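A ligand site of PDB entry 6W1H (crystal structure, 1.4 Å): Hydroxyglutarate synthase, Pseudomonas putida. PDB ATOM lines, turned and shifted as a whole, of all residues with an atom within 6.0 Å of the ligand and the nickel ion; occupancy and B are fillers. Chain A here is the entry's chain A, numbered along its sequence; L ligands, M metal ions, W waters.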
ATOM      1  N   HIS A  70      28.284  -4.177  14.028  1.00  0.00           N
ATOM      2  CA  HIS A  70      27.197  -5.155  14.078  1.00  0.00           C
ATOM      3  C   HIS A  70      25.889  -4.422  13.764  1.00  0.00           C
ATOM      4  O   HIS A  70      25.768  -3.222  13.989  1.00  0.00           O
ATOM      5  CB  HIS A  70      27.120  -6.004  15.356  1.00  0.00           C
ATOM      6  CG  HIS A  70      26.372  -5.418  16.514  1.00  0.00           C
ATOM      7  ND1 HIS A  70      27.000  -5.067  17.688  1.00  0.00           N
ATOM      8  CD2 HIS A  70      25.048  -5.229  16.723  1.00  0.00           C
ATOM      9  CE1 HIS A  70      26.104  -4.638  18.564  1.00  0.00           C
ATOM     10  NE2 HIS A  70      24.909  -4.735  18.004  1.00  0.00           N
ATOM     11  N   GLY A  71      24.962  -5.136  13.175  1.00  0.00           N
ATOM     12  CA  GLY A  71      23.606  -4.667  13.035  1.00  0.00           C
ATOM     13  C   GLY A  71      22.672  -5.568  13.802  1.00  0.00           C
ATOM     14  O   GLY A  71      23.034  -6.698  14.158  1.00  0.00           O
ATOM     15  N   ALA A  72      21.445  -5.084  14.019  1.00  0.00           N
ATOM     16  CA  ALA A  72      20.408  -5.896  14.639  1.00  0.00           C
ATOM     17  C   ALA A  72      19.119  -5.680  13.872  1.00  0.00           C
ATOM     18  O   ALA A  72      18.764  -4.549  13.561  1.00  0.00           O
ATOM     19  CB  ALA A  72      20.187  -5.480  16.096  1.00  0.00           C
ATOM     20  N   ILE A  73      18.420  -6.784  13.579  1.00  0.00           N
ATOM     21  CA  ILE A  73      17.179  -6.746  12.844  1.00  0.00           C
ATOM     22  C   ILE A  73      16.219  -7.750  13.469  1.00  0.00           C
ATOM     23  O   ILE A  73      16.620  -8.666  14.182  1.00  0.00           O
ATOM     24  CB  ILE A  73      17.340  -7.070  11.341  1.00  0.00           C
ATOM     25  CG1 ILE A  73      17.908  -8.470  11.152  1.00  0.00           C
ATOM     26  CG2 ILE A  73      18.226  -6.032  10.693  1.00  0.00           C
ATOM     27  CD1 ILE A  73      17.960  -8.917   9.700  1.00  0.00           C
ATOM     28  N   ARG A  74      14.936  -7.550  13.167  1.00  0.00           N
ATOM     29  CA  ARG A  74      13.864  -8.444  13.623  1.00  0.00           C
ATOM     30  C   ARG A  74      12.989  -8.808  12.436  1.00  0.00           C
ATOM     31  O   ARG A  74      12.628  -7.933  11.638  1.00  0.00           O
ATOM     32  CB  ARG A  74      13.010  -7.774  14.687  1.00  0.00           C
ATOM     33  CG  ARG A  74      13.771  -7.377  15.928  1.00  0.00           C
ATOM     34  CD  ARG A  74      13.589  -5.929  16.224  1.00  0.00           C
ATOM     35  NE  ARG A  74      14.186  -5.558  17.505  1.00  0.00           N
ATOM     36  CZ  ARG A  74      13.709  -4.591  18.285  1.00  0.00           C
ATOM     37  NH1 ARG A  74      12.661  -3.898  17.912  1.00  0.00           N
ATOM     38  NH2 ARG A  74      14.312  -4.330  19.424  1.00  0.00           N
ATOM     39  N   PHE A 129      22.753  -9.557  14.226  1.00  0.00           N
ATOM     40  CA  PHE A 129      21.929 -10.287  15.190  1.00  0.00           C
ATOM     41  C   PHE A 129      20.509 -10.236  14.685  1.00  0.00           C
ATOM     42  O   PHE A 129      19.976  -9.146  14.443  1.00  0.00           O
ATOM     43  CB  PHE A 129      22.043  -9.631  16.550  1.00  0.00           C
ATOM     44  CG  PHE A 129      21.431 -10.416  17.673  1.00  0.00           C
ATOM     45  CD1 PHE A 129      20.067 -10.324  17.949  1.00  0.00           C
ATOM     46  CD2 PHE A 129      22.215 -11.240  18.468  1.00  0.00           C
ATOM     47  CE1 PHE A 129      19.501 -11.028  19.018  1.00  0.00           C
ATOM     48  CE2 PHE A 129      21.658 -11.947  19.522  1.00  0.00           C
ATOM     49  CZ  PHE A 129      20.300 -11.826  19.811  1.00  0.00           C
ATOM     50  N   SER A 131      16.551 -11.566  15.046  1.00  0.00           N
ATOM     51  CA  SER A 131      15.525 -12.112  15.907  1.00  0.00           C
ATOM     52  C   SER A 131      14.284 -12.465  15.097  1.00  0.00           C
ATOM     53  O   SER A 131      13.877 -11.717  14.197  1.00  0.00           O
ATOM     54  CB  SER A 131      15.148 -11.092  16.979  1.00  0.00           C
ATOM     55  OG  SER A 131      16.215 -10.882  17.858  1.00  0.00           O
ATOM     56  N   LEU A 212       7.800  -3.846  20.595  1.00  0.00           N
ATOM     57  CA  LEU A 212       8.518  -4.667  19.630  1.00  0.00           C
ATOM     58  C   LEU A 212       7.568  -5.274  18.610  1.00  0.00           C
ATOM     59  O   LEU A 212       7.935  -5.445  17.441  1.00  0.00           O
ATOM     60  CB  LEU A 212       9.294  -5.774  20.332  1.00  0.00           C
ATOM     61  CG  LEU A 212      10.222  -6.582  19.412  1.00  0.00           C
ATOM     62  CD1 LEU A 212      11.555  -6.865  20.081  1.00  0.00           C
ATOM     63  CD2 LEU A 212       9.549  -7.868  18.996  1.00  0.00           C
ATOM     64  N   ASN A 225      17.546  -1.972  13.339  1.00  0.00           N
ATOM     65  CA  ASN A 225      17.216  -1.547  14.693  1.00  0.00           C
ATOM     66  C   ASN A 225      18.330  -0.683  15.248  1.00  0.00           C
ATOM     67  O   ASN A 225      18.068   0.293  15.946  1.00  0.00           O
ATOM     68  CB  ASN A 225      16.987  -2.757  15.597  1.00  0.00           C
ATOM     69  CG  ASN A 225      16.582  -2.349  16.983  1.00  0.00           C
ATOM     70  OD1 ASN A 225      17.423  -2.234  17.863  1.00  0.00           O
ATOM     71  ND2 ASN A 225      15.310  -2.084  17.169  1.00  0.00           N
ATOM     72  N   HIS A 226      19.580  -1.033  14.974  1.00  0.00           N
ATOM     73  CA  HIS A 226      20.727  -0.186  15.210  1.00  0.00           C
ATOM     74  C   HIS A 226      21.924  -0.795  14.482  1.00  0.00           C
ATOM     75  O   HIS A 226      21.925  -1.965  14.109  1.00  0.00           O
ATOM     76  CB  HIS A 226      20.988  -0.037  16.686  1.00  0.00           C
ATOM     77  CG  HIS A 226      21.269  -1.322  17.397  1.00  0.00           C
ATOM     78  ND1 HIS A 226      20.262  -2.090  17.938  1.00  0.00           N
ATOM     79  CD2 HIS A 226      22.417  -2.002  17.616  1.00  0.00           C
ATOM     80  CE1 HIS A 226      20.785  -3.152  18.532  1.00  0.00           C
ATOM     81  NE2 HIS A 226      22.091  -3.134  18.332  1.00  0.00           N
ATOM     82  N   THR A 228      26.102  -0.770  15.331  1.00  0.00           N
ATOM     83  CA  THR A 228      26.990  -0.496  16.452  1.00  0.00           C
ATOM     84  C   THR A 228      28.422  -0.550  15.985  1.00  0.00           C
ATOM     85  O   THR A 228      28.873  -1.612  15.528  1.00  0.00           O
ATOM     86  CB  THR A 228      26.760  -1.556  17.536  1.00  0.00           C
ATOM     87  OG1 THR A 228      25.389  -1.479  17.886  1.00  0.00           O
ATOM     88  CG2 THR A 228      27.648  -1.323  18.739  1.00  0.00           C
ATOM     89  N   LEU A 264      32.103  -8.529  25.743  1.00  0.00           N
ATOM     90  CA  LEU A 264      32.021  -7.153  25.283  1.00  0.00           C
ATOM     91  C   LEU A 264      31.361  -6.293  26.352  1.00  0.00           C
ATOM     92  O   LEU A 264      30.763  -6.800  27.305  1.00  0.00           O
ATOM     93  CB  LEU A 264      31.244  -7.043  23.972  1.00  0.00           C
ATOM     94  CG  LEU A 264      29.753  -7.369  23.955  1.00  0.00           C
ATOM     95  CD1 LEU A 264      28.918  -6.224  24.476  1.00  0.00           C
ATOM     96  CD2 LEU A 264      29.321  -7.725  22.539  1.00  0.00           C
ATOM     97  N   GLN A 266      28.909  -2.631  26.589  1.00  0.00           N
ATOM     98  CA  GLN A 266      27.957  -1.922  25.738  1.00  0.00           C
ATOM     99  C   GLN A 266      27.227  -0.851  26.515  1.00  0.00           C
ATOM    100  O   GLN A 266      27.043  -0.948  27.720  1.00  0.00           O
ATOM    101  CB  GLN A 266      26.945  -2.918  25.165  1.00  0.00           C
ATOM    102  CG  GLN A 266      25.766  -2.286  24.414  1.00  0.00           C
ATOM    103  CD  GLN A 266      24.598  -1.903  25.336  1.00  0.00           C
ATOM    104  OE1 GLN A 266      24.716  -1.942  26.572  1.00  0.00           O
ATOM    105  NE2 GLN A 266      23.472  -1.529  24.737  1.00  0.00           N
ATOM    106  N   GLU A 294      23.864   2.585  19.752  1.00  0.00           N
ATOM    107  CA  GLU A 294      24.635   1.731  20.627  1.00  0.00           C
ATOM    108  C   GLU A 294      26.120   1.842  20.301  1.00  0.00           C
ATOM    109  O   GLU A 294      26.518   2.180  19.186  1.00  0.00           O
ATOM    110  CB  GLU A 294      24.152   0.294  20.422  1.00  0.00           C
ATOM    111  CG  GLU A 294      24.798  -0.779  21.285  1.00  0.00           C
ATOM    112  CD  GLU A 294      24.071  -2.086  21.119  1.00  0.00           C
ATOM    113  OE1 GLU A 294      24.358  -2.800  20.152  1.00  0.00           O
ATOM    114  OE2 GLU A 294      23.168  -2.363  21.914  1.00  0.00           O
ATOM    115  N   GLU A 296      29.879  -0.390  21.413  1.00  0.00           N
ATOM    116  CA  GLU A 296      30.427  -1.556  22.089  1.00  0.00           C
ATOM    117  C   GLU A 296      31.947  -1.568  22.024  1.00  0.00           C
ATOM    118  O   GLU A 296      32.561  -0.947  21.164  1.00  0.00           O
ATOM    119  CB  GLU A 296      29.856  -2.869  21.534  1.00  0.00           C
ATOM    120  CG  GLU A 296      30.356  -3.272  20.171  1.00  0.00           C
ATOM    121  CD  GLU A 296      29.552  -4.420  19.568  1.00  0.00           C
ATOM    122  OE1 GLU A 296      28.703  -5.030  20.255  1.00  0.00           O
ATOM    123  OE2 GLU A 296      29.764  -4.721  18.401  1.00  0.00           O
ATOM    124  N   PHE A 399      27.388 -12.093  21.094  1.00  0.00           N
ATOM    125  CA  PHE A 399      26.563 -11.110  21.787  1.00  0.00           C
ATOM    126  C   PHE A 399      26.216 -11.576  23.203  1.00  0.00           C
ATOM    127  O   PHE A 399      26.135 -12.772  23.469  1.00  0.00           O
ATOM    128  CB  PHE A 399      25.270 -10.860  20.970  1.00  0.00           C
ATOM    129  CG  PHE A 399      25.537 -10.325  19.617  1.00  0.00           C
ATOM    130  CD1 PHE A 399      25.812 -11.175  18.557  1.00  0.00           C
ATOM    131  CD2 PHE A 399      25.530  -8.952  19.396  1.00  0.00           C
ATOM    132  CE1 PHE A 399      26.082 -10.648  17.289  1.00  0.00           C
ATOM    133  CE2 PHE A 399      25.797  -8.440  18.156  1.00  0.00           C
ATOM    134  CZ  PHE A 399      26.059  -9.280  17.093  1.00  0.00           C
ATOM    135  N   LEU A 400      26.083 -10.633  24.101  1.00  0.00           N
ATOM    136  CA  LEU A 400      25.776 -10.970  25.498  1.00  0.00           C
ATOM    137  C   LEU A 400      24.478 -11.750  25.644  1.00  0.00           C
ATOM    138  O   LEU A 400      24.484 -12.724  26.406  1.00  0.00           O
ATOM    139  CB  LEU A 400      25.801  -9.713  26.365  1.00  0.00           C
ATOM    140  CG  LEU A 400      27.121  -8.972  26.465  1.00  0.00           C
ATOM    141  CD1 LEU A 400      26.911  -7.698  27.307  1.00  0.00           C
ATOM    142  CD2 LEU A 400      28.193  -9.833  27.026  1.00  0.00           C
ATOM    143  N   PRO A 401      23.337 -11.356  25.046  1.00  0.00           N
ATOM    144  CA  PRO A 401      23.051 -10.137  24.262  1.00  0.00           C
ATOM    145  C   PRO A 401      22.430  -9.012  25.104  1.00  0.00           C
ATOM    146  O   PRO A 401      22.057  -9.210  26.265  1.00  0.00           O
ATOM    147  CB  PRO A 401      21.995 -10.631  23.275  1.00  0.00           C
ATOM    148  CG  PRO A 401      21.172 -11.611  24.103  1.00  0.00           C
ATOM    149  CD  PRO A 401      22.132 -12.220  25.121  1.00  0.00           C
ATOM    150  N   VAL A 402      22.274  -7.820  24.535  1.00  0.00           N
ATOM    151  CA  VAL A 402      21.760  -6.602  25.179  1.00  0.00           C
ATOM    152  C   VAL A 402      20.880  -5.899  24.162  1.00  0.00           C
ATOM    153  O   VAL A 402      21.007  -6.072  23.051  1.00  0.00           O
ATOM    154  CB  VAL A 402      22.930  -5.706  25.668  1.00  0.00           C
ATOM    155  CG1 VAL A 402      23.799  -5.177  24.535  1.00  0.00           C
ATOM    156  CG2 VAL A 402      22.453  -4.551  26.545  1.00  0.00           C
ATOM    157  N   SER A 403      19.896  -5.176  24.596  1.00  0.00           N
ATOM    158  CA  SER A 403      18.979  -4.449  23.722  1.00  0.00           C
ATOM    159  C   SER A 403      19.182  -2.951  23.889  1.00  0.00           C
ATOM    160  O   SER A 403      18.976  -2.410  24.984  1.00  0.00           O
ATOM    161  CB  SER A 403      17.521  -4.816  24.028  1.00  0.00           C
ATOM    162  OG  SER A 403      16.631  -4.253  23.062  1.00  0.00           O
ATOM    163  N   ALA A 404      19.569  -2.289  22.800  1.00  0.00           N
ATOM    164  CA  ALA A 404      19.706  -0.843  22.847  1.00  0.00           C
ATOM    165  C   ALA A 404      18.378  -0.154  23.137  1.00  0.00           C
ATOM    166  O   ALA A 404      18.356   0.907  23.769  1.00  0.00           O
ATOM    167  CB  ALA A 404      20.292  -0.319  21.533  1.00  0.00           C
ATOM    168  N   ALA A 405      17.278  -0.729  22.664  1.00  0.00           N
ATOM    169  CA  ALA A 405      15.946  -0.165  22.865  1.00  0.00           C
ATOM    170  C   ALA A 405      15.314  -0.627  24.173  1.00  0.00           C
ATOM    171  O   ALA A 405      14.151  -0.311  24.410  1.00  0.00           O
ATOM    172  CB  ALA A 405      15.037  -0.514  21.682  1.00  0.00           C
ATOM    173  N   ILE A 407      14.461  -3.760  25.259  1.00  0.00           N
ATOM    174  CA  ILE A 407      13.373  -4.726  25.101  1.00  0.00           C
ATOM    175  C   ILE A 407      13.506  -5.880  26.087  1.00  0.00           C
ATOM    176  O   ILE A 407      12.502  -6.362  26.623  1.00  0.00           O
ATOM    177  CB  ILE A 407      13.308  -5.210  23.638  1.00  0.00           C
ATOM    178  CG1 ILE A 407      13.075  -4.052  22.678  1.00  0.00           C
ATOM    179  CG2 ILE A 407      12.197  -6.255  23.472  1.00  0.00           C
ATOM    180  CD1 ILE A 407      11.793  -3.278  22.928  1.00  0.00           C
ATOM    181  N   PHE A 408      14.730  -6.338  26.343  1.00  0.00           N
ATOM    182  CA  PHE A 408      14.947  -7.468  27.241  1.00  0.00           C
ATOM    183  C   PHE A 408      16.095  -7.159  28.201  1.00  0.00           C
ATOM    184  O   PHE A 408      16.919  -6.277  27.958  1.00  0.00           O
ATOM    185  CB  PHE A 408      15.256  -8.764  26.477  1.00  0.00           C
ATOM    186  CG  PHE A 408      16.297  -8.617  25.399  1.00  0.00           C
ATOM    187  CD1 PHE A 408      17.649  -8.722  25.693  1.00  0.00           C
ATOM    188  CD2 PHE A 408      15.917  -8.393  24.086  1.00  0.00           C
ATOM    189  CE1 PHE A 408      18.601  -8.596  24.694  1.00  0.00           C
ATOM    190  CE2 PHE A 408      16.866  -8.254  23.083  1.00  0.00           C
ATOM    191  CZ  PHE A 408      18.201  -8.368  23.389  1.00  0.00           C
HETATM  192  C1  LIG L   1      18.851  -6.302  20.328  1.00  0.00           C
HETATM  193  C2  LIG L   1      19.557  -7.374  19.522  1.00  0.00           C
HETATM  194  C3  LIG L   1      20.843  -7.806  20.202  1.00  0.00           C
HETATM  195  C4  LIG L   1      23.159  -6.768  20.890  1.00  0.00           C
HETATM  196  O1  LIG L   1      23.314  -7.705  21.743  1.00  0.00           O
HETATM  197  O2  LIG L   1      23.969  -5.796  20.781  1.00  0.00           O
HETATM  198  C5  LIG L   1      21.966  -6.784  19.961  1.00  0.00           C
HETATM  199  C6  LIG L   1      17.430  -6.039  19.807  1.00  0.00           C
HETATM  200  O3  LIG L   1      16.685  -5.345  20.428  1.00  0.00           O
HETATM  201  O4  LIG L   1      16.963  -6.600  18.610  1.00  0.00           O
HETATM  202  O5  LIG L   1      21.966  -6.007  19.053  1.00  0.00           O
HETATM  203 NI    NI M   1      23.285  -4.391  19.460  1.00  0.00          NI
HETATM  204  O   HOH W   1      26.302  -5.232  22.273  1.00  0.00           O
HETATM  205  O   HOH W   2      17.754  -2.803  20.404  1.00  0.00           O
HETATM  206  O   HOH W   3      21.656  -4.022  21.231  1.00  0.00           O
HETATM  207  O   HOH W   4      17.326  -8.688  16.935  1.00  0.00           O
HETATM  208  O   HOH W   5      25.686  -7.942  23.111  1.00  0.00           O
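The nickel ion is bound by the side-chain carboxylate of Glu 294 (2.0 Å), an oxygen (O2) of the ligand (2.0 Å), a ring nitrogen (NE2) of His 226 (2.1 Å), an oxygen (O5) of the ligand (2.1 Å), a ring nitrogen (NE2) of His 70 (2.2 Å) and water W3 (2.4 Å).
The nickel ion has six donor atoms within binding distance.
The side-chain carboxylate of Glu 294 sits close to the side-chain hydroxyl of Thr 228 (2.8 Å).
NE2 of Gln 266 sits at hydrogen-bond distance from OE2 of Glu 294, 3.0 Å away.
ND1 of His 226 sits at hydrogen-bond distance from OD1 of Asn 225 (2.8 Å).
The backbone carbonyl oxygen (O) of His 70 sits at hydrogen-bond distance from the backbone NH (N) of Thr 228.
The guanidinium group of Arg 74 sits close to the side-chain amide nitrogen of Asn 225, at 3.3 Å.
The side-chain hydroxyl of Ser 403 is in hydrogen-bond range of the backbone NH of Ile 407, at 3.1 Å.
The backbone carbonyl oxygen (O) of Gly 71 sits at hydrogen-bond distance from the backbone NH (N) of Phe 129 (2.9 Å).
N of Asn 225 sits at hydrogen-bond distance from O of Ala 72, at 2.9 Å.
Merely in contact with the nickel ion: Thr 228 (3.9 Å).
Four residues have an atom within 4 Å of the nickel ion: His 70, His 226, Thr 228 and Glu 294.
The nearest printed residue that does not touch the nickel ion is Val 402 (4.6 Å).
Water W4 lies within hydrogen-bond range of OG of Ser 131, O4 of the ligand and O of Ile 73.
Water W5 lies within hydrogen-bond range of O1 of the ligand (2.7 Å) and N of Leu 400 (2.9 Å).
Water W2 lies within hydrogen-bond range of OD1 of Asn 225, O3 of the ligand, N of Ala 404, N of Ala 405 and OG of Ser 403.
Residues that only touch the ligand: Phe 129, Phe 399, Ala 72, Pro 401 and Phe 408.
Hydrophobic or aromatic side chains that line the ligand: His 70, Ala 72, Phe 129, His 226, Phe 399, Pro 401, Val 402 and Phe 408.
11 residues have an atom within 4 Å of the ligand: His 70, Ala 72, Arg 74, Phe 129, His 226, Glu 294, Phe 399, Pro 401, Val 402, Ser 403 and Phe 408.
The nearest printed residue that does not touch the ligand is Asn 225 (4.1 Å).
NH2 of Arg 74 lies within salt-bridge range of O3 of the ligand.
The side-chain hydroxyl (OG) of Ser 403 is in hydrogen-bond range of an oxygen (O3) of the ligand (2.9 Å).
An oxygen (O1) of the ligand is in hydrogen-bond range of the backbone NH (N) of Val 402 (3.0 Å).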
